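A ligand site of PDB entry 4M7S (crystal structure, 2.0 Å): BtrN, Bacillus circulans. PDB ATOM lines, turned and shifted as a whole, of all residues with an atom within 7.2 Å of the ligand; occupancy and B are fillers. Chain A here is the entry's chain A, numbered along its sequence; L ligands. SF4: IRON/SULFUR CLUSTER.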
ATOM      1  N   LYS A 164     -11.884  22.009  18.036  1.00  0.00           N
ATOM      2  CA  LYS A 164     -13.054  21.272  17.548  1.00  0.00           C
ATOM      3  C   LYS A 164     -13.028  19.808  17.964  1.00  0.00           C
ATOM      4  O   LYS A 164     -14.000  19.080  17.779  1.00  0.00           O
ATOM      5  CB  LYS A 164     -13.151  21.381  16.022  1.00  0.00           C
ATOM      6  N   MET A 167     -15.989  18.832  20.111  1.00  0.00           N
ATOM      7  CA  MET A 167     -17.329  19.217  19.717  1.00  0.00           C
ATOM      8  C   MET A 167     -18.174  18.019  19.332  1.00  0.00           C
ATOM      9  O   MET A 167     -17.697  17.078  18.702  1.00  0.00           O
ATOM     10  CB  MET A 167     -17.309  20.176  18.527  1.00  0.00           C
ATOM     11  CG  MET A 167     -16.646  21.494  18.809  1.00  0.00           C
ATOM     12  SD  MET A 167     -17.235  22.844  17.532  1.00  0.00           S
ATOM     13  CE  MET A 167     -15.558  23.825  17.354  1.00  0.00           C
ATOM     14  N   SER A 168     -19.435  18.064  19.722  1.00  0.00           N
ATOM     15  CA  SER A 168     -20.393  17.046  19.311  1.00  0.00           C
ATOM     16  C   SER A 168     -20.718  17.217  17.833  1.00  0.00           C
ATOM     17  O   SER A 168     -20.445  18.266  17.233  1.00  0.00           O
ATOM     18  CB  SER A 168     -21.682  17.194  20.099  1.00  0.00           C
ATOM     19  OG  SER A 168     -22.386  18.344  19.651  1.00  0.00           O
ATOM     20  N   CYS A 169     -21.304  16.193  17.243  1.00  0.00           N
ATOM     21  CA  CYS A 169     -21.903  16.320  15.928  1.00  0.00           C
ATOM     22  C   CYS A 169     -22.944  15.248  15.704  1.00  0.00           C
ATOM     23  O   CYS A 169     -22.678  14.067  15.876  1.00  0.00           O
ATOM     24  CB  CYS A 169     -20.856  16.235  14.822  1.00  0.00           C
ATOM     25  SG  CYS A 169     -21.671  16.359  13.216  1.00  0.00           S
ATOM     26  N   MET A 170     -24.119  15.690  15.284  1.00  0.00           N
ATOM     27  CA  MET A 170     -25.270  14.804  15.150  1.00  0.00           C
ATOM     28  C   MET A 170     -25.505  14.363  13.707  1.00  0.00           C
ATOM     29  O   MET A 170     -26.432  13.597  13.457  1.00  0.00           O
ATOM     30  CB  MET A 170     -26.535  15.493  15.678  1.00  0.00           C
ATOM     31  CG  MET A 170     -26.367  16.159  17.036  1.00  0.00           C
ATOM     32  SD  MET A 170     -25.664  14.932  18.369  1.00  0.00           S
ATOM     33  CE  MET A 170     -26.967  13.502  18.116  1.00  0.00           C
ATOM     34  N   VAL A 171     -24.686  14.821  12.774  1.00  0.00           N
ATOM     35  CA  VAL A 171     -24.859  14.421  11.354  1.00  0.00           C
ATOM     36  C   VAL A 171     -24.929  12.895  11.169  1.00  0.00           C
ATOM     37  O   VAL A 171     -25.853  12.402  10.514  1.00  0.00           O
ATOM     38  CB  VAL A 171     -23.801  15.048  10.416  1.00  0.00           C
ATOM     39  CG1 VAL A 171     -24.035  14.594   8.948  1.00  0.00           C
ATOM     40  CG2 VAL A 171     -23.829  16.573  10.508  1.00  0.00           C
ATOM     41  N   PRO A 172     -23.978  12.139  11.762  1.00  0.00           N
ATOM     42  CA  PRO A 172     -24.082  10.684  11.579  1.00  0.00           C
ATOM     43  C   PRO A 172     -25.312  10.059  12.258  1.00  0.00           C
ATOM     44  O   PRO A 172     -25.572   8.878  12.023  1.00  0.00           O
ATOM     45  CB  PRO A 172     -22.810  10.133  12.249  1.00  0.00           C
ATOM     46  CG  PRO A 172     -21.879  11.307  12.336  1.00  0.00           C
ATOM     47  CD  PRO A 172     -22.761  12.511  12.514  1.00  0.00           C
ATOM     48  N   PRO A 186     -21.250   8.394   6.477  1.00  0.00           N
ATOM     49  CA  PRO A 186     -21.987   8.950   7.614  1.00  0.00           C
ATOM     50  C   PRO A 186     -22.169  10.452   7.517  1.00  0.00           C
ATOM     51  O   PRO A 186     -22.817  11.024   8.391  1.00  0.00           O
ATOM     52  CB  PRO A 186     -21.051   8.632   8.795  1.00  0.00           C
ATOM     53  CG  PRO A 186     -19.699   8.740   8.207  1.00  0.00           C
ATOM     54  CD  PRO A 186     -19.827   8.183   6.798  1.00  0.00           C
ATOM     55  N   CYS A 187     -21.625  11.080   6.480  1.00  0.00           N
ATOM     56  CA  CYS A 187     -21.640  12.545   6.397  1.00  0.00           C
ATOM     57  C   CYS A 187     -21.348  13.112   4.993  1.00  0.00           C
ATOM     58  O   CYS A 187     -20.664  12.486   4.188  1.00  0.00           O
ATOM     59  CB  CYS A 187     -20.599  13.118   7.361  1.00  0.00           C
ATOM     60  SG  CYS A 187     -20.387  14.867   7.136  1.00  0.00           S
ATOM     61  N   PHE A 188     -21.862  14.314   4.738  1.00  0.00           N
ATOM     62  CA  PHE A 188     -21.721  14.954   3.431  1.00  0.00           C
ATOM     63  C   PHE A 188     -20.296  15.483   3.248  1.00  0.00           C
ATOM     64  O   PHE A 188     -19.911  15.883   2.140  1.00  0.00           O
ATOM     65  CB  PHE A 188     -22.705  16.134   3.329  1.00  0.00           C
ATOM     66  CG  PHE A 188     -22.655  17.045   4.517  1.00  0.00           C
ATOM     67  CD1 PHE A 188     -21.670  18.018   4.628  1.00  0.00           C
ATOM     68  CD2 PHE A 188     -23.566  16.892   5.560  1.00  0.00           C
ATOM     69  CE1 PHE A 188     -21.610  18.848   5.746  1.00  0.00           C
ATOM     70  CE2 PHE A 188     -23.511  17.723   6.670  1.00  0.00           C
ATOM     71  CZ  PHE A 188     -22.530  18.705   6.761  1.00  0.00           C
ATOM     72  N   GLU A 189     -19.536  15.504   4.334  1.00  0.00           N
ATOM     73  CA  GLU A 189     -18.147  15.959   4.320  1.00  0.00           C
ATOM     74  C   GLU A 189     -17.192  14.896   3.791  1.00  0.00           C
ATOM     75  O   GLU A 189     -16.106  15.219   3.308  1.00  0.00           O
ATOM     76  CB  GLU A 189     -17.702  16.351   5.738  1.00  0.00           C
ATOM     77  CG  GLU A 189     -18.332  17.631   6.283  1.00  0.00           C
ATOM     78  CD  GLU A 189     -17.651  18.893   5.755  1.00  0.00           C
ATOM     79  OE1 GLU A 189     -16.422  18.861   5.490  1.00  0.00           O
ATOM     80  OE2 GLU A 189     -18.354  19.912   5.602  1.00  0.00           O
ATOM     81  N   ASP A 190     -17.597  13.632   3.872  1.00  0.00           N
ATOM     82  CA  ASP A 190     -16.704  12.521   3.553  1.00  0.00           C
ATOM     83  C   ASP A 190     -16.487  12.316   2.039  1.00  0.00           C
ATOM     84  O   ASP A 190     -16.718  11.239   1.500  1.00  0.00           O
ATOM     85  CB  ASP A 190     -17.259  11.232   4.167  1.00  0.00           C
ATOM     86  CG  ASP A 190     -16.201  10.149   4.289  1.00  0.00           C
ATOM     87  OD1 ASP A 190     -15.001  10.469   4.076  1.00  0.00           O
ATOM     88  OD2 ASP A 190     -16.570   9.005   4.613  1.00  0.00           O
ATOM     89  N   PHE A 217     -19.744   4.958  15.619  1.00  0.00           N
ATOM     90  CA  PHE A 217     -19.316   6.244  15.070  1.00  0.00           C
ATOM     91  C   PHE A 217     -20.275   7.334  15.497  1.00  0.00           C
ATOM     92  O   PHE A 217     -19.853   8.387  15.966  1.00  0.00           O
ATOM     93  CB  PHE A 217     -19.217   6.189  13.544  1.00  0.00           C
ATOM     94  CG  PHE A 217     -18.669   7.451  12.919  1.00  0.00           C
ATOM     95  CD1 PHE A 217     -17.326   7.785  13.042  1.00  0.00           C
ATOM     96  CD2 PHE A 217     -19.500   8.300  12.201  1.00  0.00           C
ATOM     97  CE1 PHE A 217     -16.821   8.938  12.461  1.00  0.00           C
ATOM     98  CE2 PHE A 217     -19.000   9.462  11.600  1.00  0.00           C
ATOM     99  CZ  PHE A 217     -17.664   9.780  11.738  1.00  0.00           C
ATOM    100  N   LEU A 221     -19.454  10.478  17.990  1.00  0.00           N
ATOM    101  CA  LEU A 221     -19.614  11.872  17.568  1.00  0.00           C
ATOM    102  C   LEU A 221     -20.718  12.586  18.364  1.00  0.00           C
ATOM    103  O   LEU A 221     -20.663  13.807  18.550  1.00  0.00           O
ATOM    104  CB  LEU A 221     -19.886  11.973  16.066  1.00  0.00           C
ATOM    105  CG  LEU A 221     -18.672  12.151  15.157  1.00  0.00           C
ATOM    106  CD1 LEU A 221     -17.828  13.322  15.635  1.00  0.00           C
ATOM    107  CD2 LEU A 221     -17.836  10.896  15.120  1.00  0.00           C
ATOM    108  N   ARG A 226     -14.578  13.939  18.240  1.00  0.00           N
ATOM    109  CA  ARG A 226     -14.158  14.221  16.869  1.00  0.00           C
ATOM    110  C   ARG A 226     -12.692  13.887  16.652  1.00  0.00           C
ATOM    111  O   ARG A 226     -12.313  13.377  15.594  1.00  0.00           O
ATOM    112  CB  ARG A 226     -14.352  15.701  16.544  1.00  0.00           C
ATOM    113  CG  ARG A 226     -15.790  16.098  16.303  1.00  0.00           C
ATOM    114  CD  ARG A 226     -15.850  17.451  15.632  1.00  0.00           C
ATOM    115  NE  ARG A 226     -17.207  17.988  15.644  1.00  0.00           N
ATOM    116  CZ  ARG A 226     -17.579  19.092  15.004  1.00  0.00           C
ATOM    117  NH1 ARG A 226     -18.830  19.511  15.074  1.00  0.00           N
ATOM    118  NH2 ARG A 226     -16.693  19.770  14.290  1.00  0.00           N
ATOM    119  N   SER A 229     -11.659  10.429  15.218  1.00  0.00           N
ATOM    120  CA  SER A 229     -11.990  10.084  13.840  1.00  0.00           C
ATOM    121  C   SER A 229     -11.105  10.822  12.826  1.00  0.00           C
ATOM    122  O   SER A 229     -10.949  12.029  12.892  1.00  0.00           O
ATOM    123  CB  SER A 229     -13.449  10.455  13.564  1.00  0.00           C
ATOM    124  OG  SER A 229     -13.690  10.414  12.174  1.00  0.00           O
ATOM    125  N   LEU A 231     -11.918  11.334   9.887  1.00  0.00           N
ATOM    126  CA  LEU A 231     -12.858  12.164   9.139  1.00  0.00           C
ATOM    127  C   LEU A 231     -13.069  13.464   9.901  1.00  0.00           C
ATOM    128  O   LEU A 231     -12.920  14.554   9.344  1.00  0.00           O
ATOM    129  CB  LEU A 231     -14.198  11.441   9.013  1.00  0.00           C
ATOM    130  CG  LEU A 231     -15.116  11.620   7.801  1.00  0.00           C
ATOM    131  CD1 LEU A 231     -16.581  11.349   8.177  1.00  0.00           C
ATOM    132  CD2 LEU A 231     -14.934  12.955   7.052  1.00  0.00           C
ATOM    133  N   CYS A 232     -13.406  13.351  11.186  1.00  0.00           N
ATOM    134  CA  CYS A 232     -13.920  14.503  11.945  1.00  0.00           C
ATOM    135  C   CYS A 232     -12.891  15.377  12.632  1.00  0.00           C
ATOM    136  O   CYS A 232     -13.154  16.559  12.903  1.00  0.00           O
ATOM    137  CB  CYS A 232     -14.937  14.011  12.985  1.00  0.00           C
ATOM    138  SG  CYS A 232     -16.224  12.980  12.233  1.00  0.00           S
ATOM    139  N   LYS A 233     -11.713  14.836  12.927  1.00  0.00           N
ATOM    140  CA  LYS A 233     -10.743  15.523  13.766  1.00  0.00           C
ATOM    141  C   LYS A 233     -10.291  16.887  13.219  1.00  0.00           C
ATOM    142  O   LYS A 233      -9.881  17.759  13.975  1.00  0.00           O
ATOM    143  CB  LYS A 233      -9.538  14.622  14.045  1.00  0.00           C
ATOM    144  CG  LYS A 233      -8.699  14.312  12.815  1.00  0.00           C
ATOM    145  CD  LYS A 233      -7.654  13.254  13.122  1.00  0.00           C
ATOM    146  CE  LYS A 233      -6.652  13.149  11.983  1.00  0.00           C
ATOM    147  NZ  LYS A 233      -5.656  12.066  12.235  1.00  0.00           N
ATOM    148  N   ASN A 234     -10.379  17.068  11.903  1.00  0.00           N
ATOM    149  CA  ASN A 234      -9.994  18.337  11.296  1.00  0.00           C
ATOM    150  C   ASN A 234     -11.203  19.078  10.740  1.00  0.00           C
ATOM    151  O   ASN A 234     -11.064  20.097  10.067  1.00  0.00           O
ATOM    152  CB  ASN A 234      -8.956  18.116  10.209  1.00  0.00           C
ATOM    153  CG  ASN A 234      -7.646  17.608  10.766  1.00  0.00           C
ATOM    154  OD1 ASN A 234      -7.204  18.050  11.826  1.00  0.00           O
ATOM    155  ND2 ASN A 234      -7.026  16.670  10.073  1.00  0.00           N
ATOM    156  N   CYS A 235     -12.404  18.563  11.035  1.00  0.00           N
ATOM    157  CA  CYS A 235     -13.614  19.200  10.555  1.00  0.00           C
ATOM    158  C   CYS A 235     -13.957  20.480  11.302  1.00  0.00           C
ATOM    159  O   CYS A 235     -13.914  20.524  12.542  1.00  0.00           O
ATOM    160  CB  CYS A 235     -14.816  18.265  10.648  1.00  0.00           C
ATOM    161  SG  CYS A 235     -16.270  19.086   9.965  1.00  0.00           S
ATOM    162  N   ASN A 236     -14.340  21.506  10.558  1.00  0.00           N
ATOM    163  CA  ASN A 236     -14.730  22.782  11.146  1.00  0.00           C
ATOM    164  C   ASN A 236     -16.231  23.050  11.052  1.00  0.00           C
ATOM    165  O   ASN A 236     -16.661  24.204  10.977  1.00  0.00           O
ATOM    166  CB  ASN A 236     -13.954  23.924  10.493  1.00  0.00           C
ATOM    167  CG  ASN A 236     -13.910  23.804   8.996  1.00  0.00           C
ATOM    168  OD1 ASN A 236     -14.640  22.986   8.413  1.00  0.00           O
ATOM    169  ND2 ASN A 236     -13.063  24.598   8.349  1.00  0.00           N
ATOM    170  N   ASN A 237     -17.023  21.983  11.064  1.00  0.00           N
ATOM    171  CA  ASN A 237     -18.456  22.158  11.204  1.00  0.00           C
ATOM    172  C   ASN A 237     -18.788  22.546  12.635  1.00  0.00           C
ATOM    173  O   ASN A 237     -18.526  21.786  13.563  1.00  0.00           O
ATOM    174  CB  ASN A 237     -19.218  20.880  10.856  1.00  0.00           C
ATOM    175  CG  ASN A 237     -20.690  20.978  11.214  1.00  0.00           C
ATOM    176  OD1 ASN A 237     -21.308  22.030  11.082  1.00  0.00           O
ATOM    177  ND2 ASN A 237     -21.267  19.861  11.677  1.00  0.00           N
ATOM    178  N   VAL A 238     -19.368  23.728  12.805  1.00  0.00           N
ATOM    179  CA  VAL A 238     -19.772  24.194  14.120  1.00  0.00           C
ATOM    180  C   VAL A 238     -21.268  24.515  14.191  1.00  0.00           C
ATOM    181  O   VAL A 238     -21.808  24.720  15.280  1.00  0.00           O
ATOM    182  CB  VAL A 238     -18.971  25.445  14.572  1.00  0.00           C
ATOM    183  CG1 VAL A 238     -17.487  25.140  14.579  1.00  0.00           C
ATOM    184  CG2 VAL A 238     -19.265  26.628  13.668  1.00  0.00           C
ATOM    185  N   VAL A 240     -23.793  22.943  11.859  1.00  0.00           N
ATOM    186  CA  VAL A 240     -24.661  21.889  11.321  1.00  0.00           C
ATOM    187  C   VAL A 240     -24.798  20.698  12.262  1.00  0.00           C
ATOM    188  O   VAL A 240     -23.883  19.892  12.394  1.00  0.00           O
ATOM    189  CB  VAL A 240     -24.143  21.412   9.947  1.00  0.00           C
ATOM    190  CG1 VAL A 240     -25.115  20.399   9.334  1.00  0.00           C
ATOM    191  CG2 VAL A 240     -23.944  22.602   9.026  1.00  0.00           C
ATOM    192  N   GLN A 241     -25.958  20.599  12.922  1.00  0.00           N
ATOM    193  CA  GLN A 241     -26.272  19.502  13.836  1.00  0.00           C
ATOM    194  C   GLN A 241     -25.249  19.301  14.949  1.00  0.00           C
ATOM    195  O   GLN A 241     -24.766  18.186  15.182  1.00  0.00           O
ATOM    196  CB  GLN A 241     -26.535  18.198  13.068  1.00  0.00           C
ATOM    197  CG  GLN A 241     -27.767  18.259  12.178  1.00  0.00           C
ATOM    198  CD  GLN A 241     -28.065  16.935  11.489  1.00  0.00           C
ATOM    199  OE1 GLN A 241     -27.789  15.867  12.025  1.00  0.00           O
ATOM    200  NE2 GLN A 241     -28.649  17.012  10.302  1.00  0.00           N
ATOM    201  N   THR A 242     -24.923  20.391  15.630  1.00  0.00           N
ATOM    202  CA  THR A 242     -24.028  20.351  16.772  1.00  0.00           C
ATOM    203  C   THR A 242     -24.752  20.967  17.975  1.00  0.00           C
ATOM    204  O   THR A 242     -25.652  21.791  17.787  1.00  0.00           O
ATOM    205  CB  THR A 242     -22.732  21.129  16.471  1.00  0.00           C
ATOM    206  OG1 THR A 242     -23.017  22.536  16.431  1.00  0.00           O
ATOM    207  CG2 THR A 242     -22.129  20.692  15.131  1.00  0.00           C
HETATM  208 FE1  SF4 L   1     -17.678  17.107  10.453  1.00  0.00          FE
HETATM  209 FE2  SF4 L   1     -17.537  14.567  11.304  1.00  0.00          FE
HETATM  210 FE3  SF4 L   1     -19.149  15.239   9.267  1.00  0.00          FE
HETATM  211 FE4  SF4 L   1     -19.735  15.944  11.773  1.00  0.00          FE
HETATM  212  S1  SF4 L   1     -19.679  13.776  10.967  1.00  0.00           S
HETATM  213  S2  SF4 L   1     -19.902  17.312   9.939  1.00  0.00           S
HETATM  214  S3  SF4 L   1     -17.669  16.412  12.638  1.00  0.00           S
HETATM  215  S4  SF4 L   1     -16.852  15.345   9.220  1.00  0.00           S
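An iron atom (FE3) of the ligand is bound by the side-chain sulfur (SG) of Cys 187 (2.5 Å).
ND2 of Asn 237 lies close to S2 of the ligand, at 3.4 Å.
The side-chain sulfur (SG) of Cys 169 is bound to an iron atom (FE4) of the ligand (2.5 Å).
SG of Cys 232 binds FE2 of the ligand (2.3 Å).
The guanidinium group (NE) of Arg 226 sits close to a sulfur (S3) of the ligand, 3.4 Å away.
SG of Cys 235 binds FE1 of the ligand.
NH2 of Arg 226 sits at hydrogen-bond distance from O of Cys 235 (3.4 Å).
The backbone NH (N) of Leu 231 is in hydrogen-bond range of the side-chain hydroxyl (OG) of Ser 229.
N of Cys 232 lies within hydrogen-bond range of OG of Ser 229, at 3.1 Å.
The guanidinium group (NH1) of Arg 226 lies within hydrogen-bond range of the backbone carbonyl oxygen (O) of Ser 168 (3.0 Å).
ND2 of Asn 237 is in hydrogen-bond range of O of Val 240, at 2.7 Å.
N of Val 171 sits close to SG of Cys 169.
The guanidinium group of Arg 226 lies close to the backbone carbonyl oxygen of Met 167 (3.2 Å).
O of Asn 237 lies within hydrogen-bond range of NH1 of Arg 226 (2.7 Å).
Pro 172 touches the ligand.
CB of Glu 189 touches S4 of the ligand, 3.7 Å away.
Leu 231 touches the ligand.
Hydrophobic or aromatic side chains within 4 Å of the ligand: Pro 172 and Leu 231.
Within 4 Å of the ligand: Cys 169, Pro 172, Cys 187, Glu 189, Arg 226, Leu 231, Cys 232, Cys 235 and Asn 237.
The nearest printed residue that does not touch the ligand is Val 171 (4.04 Å).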
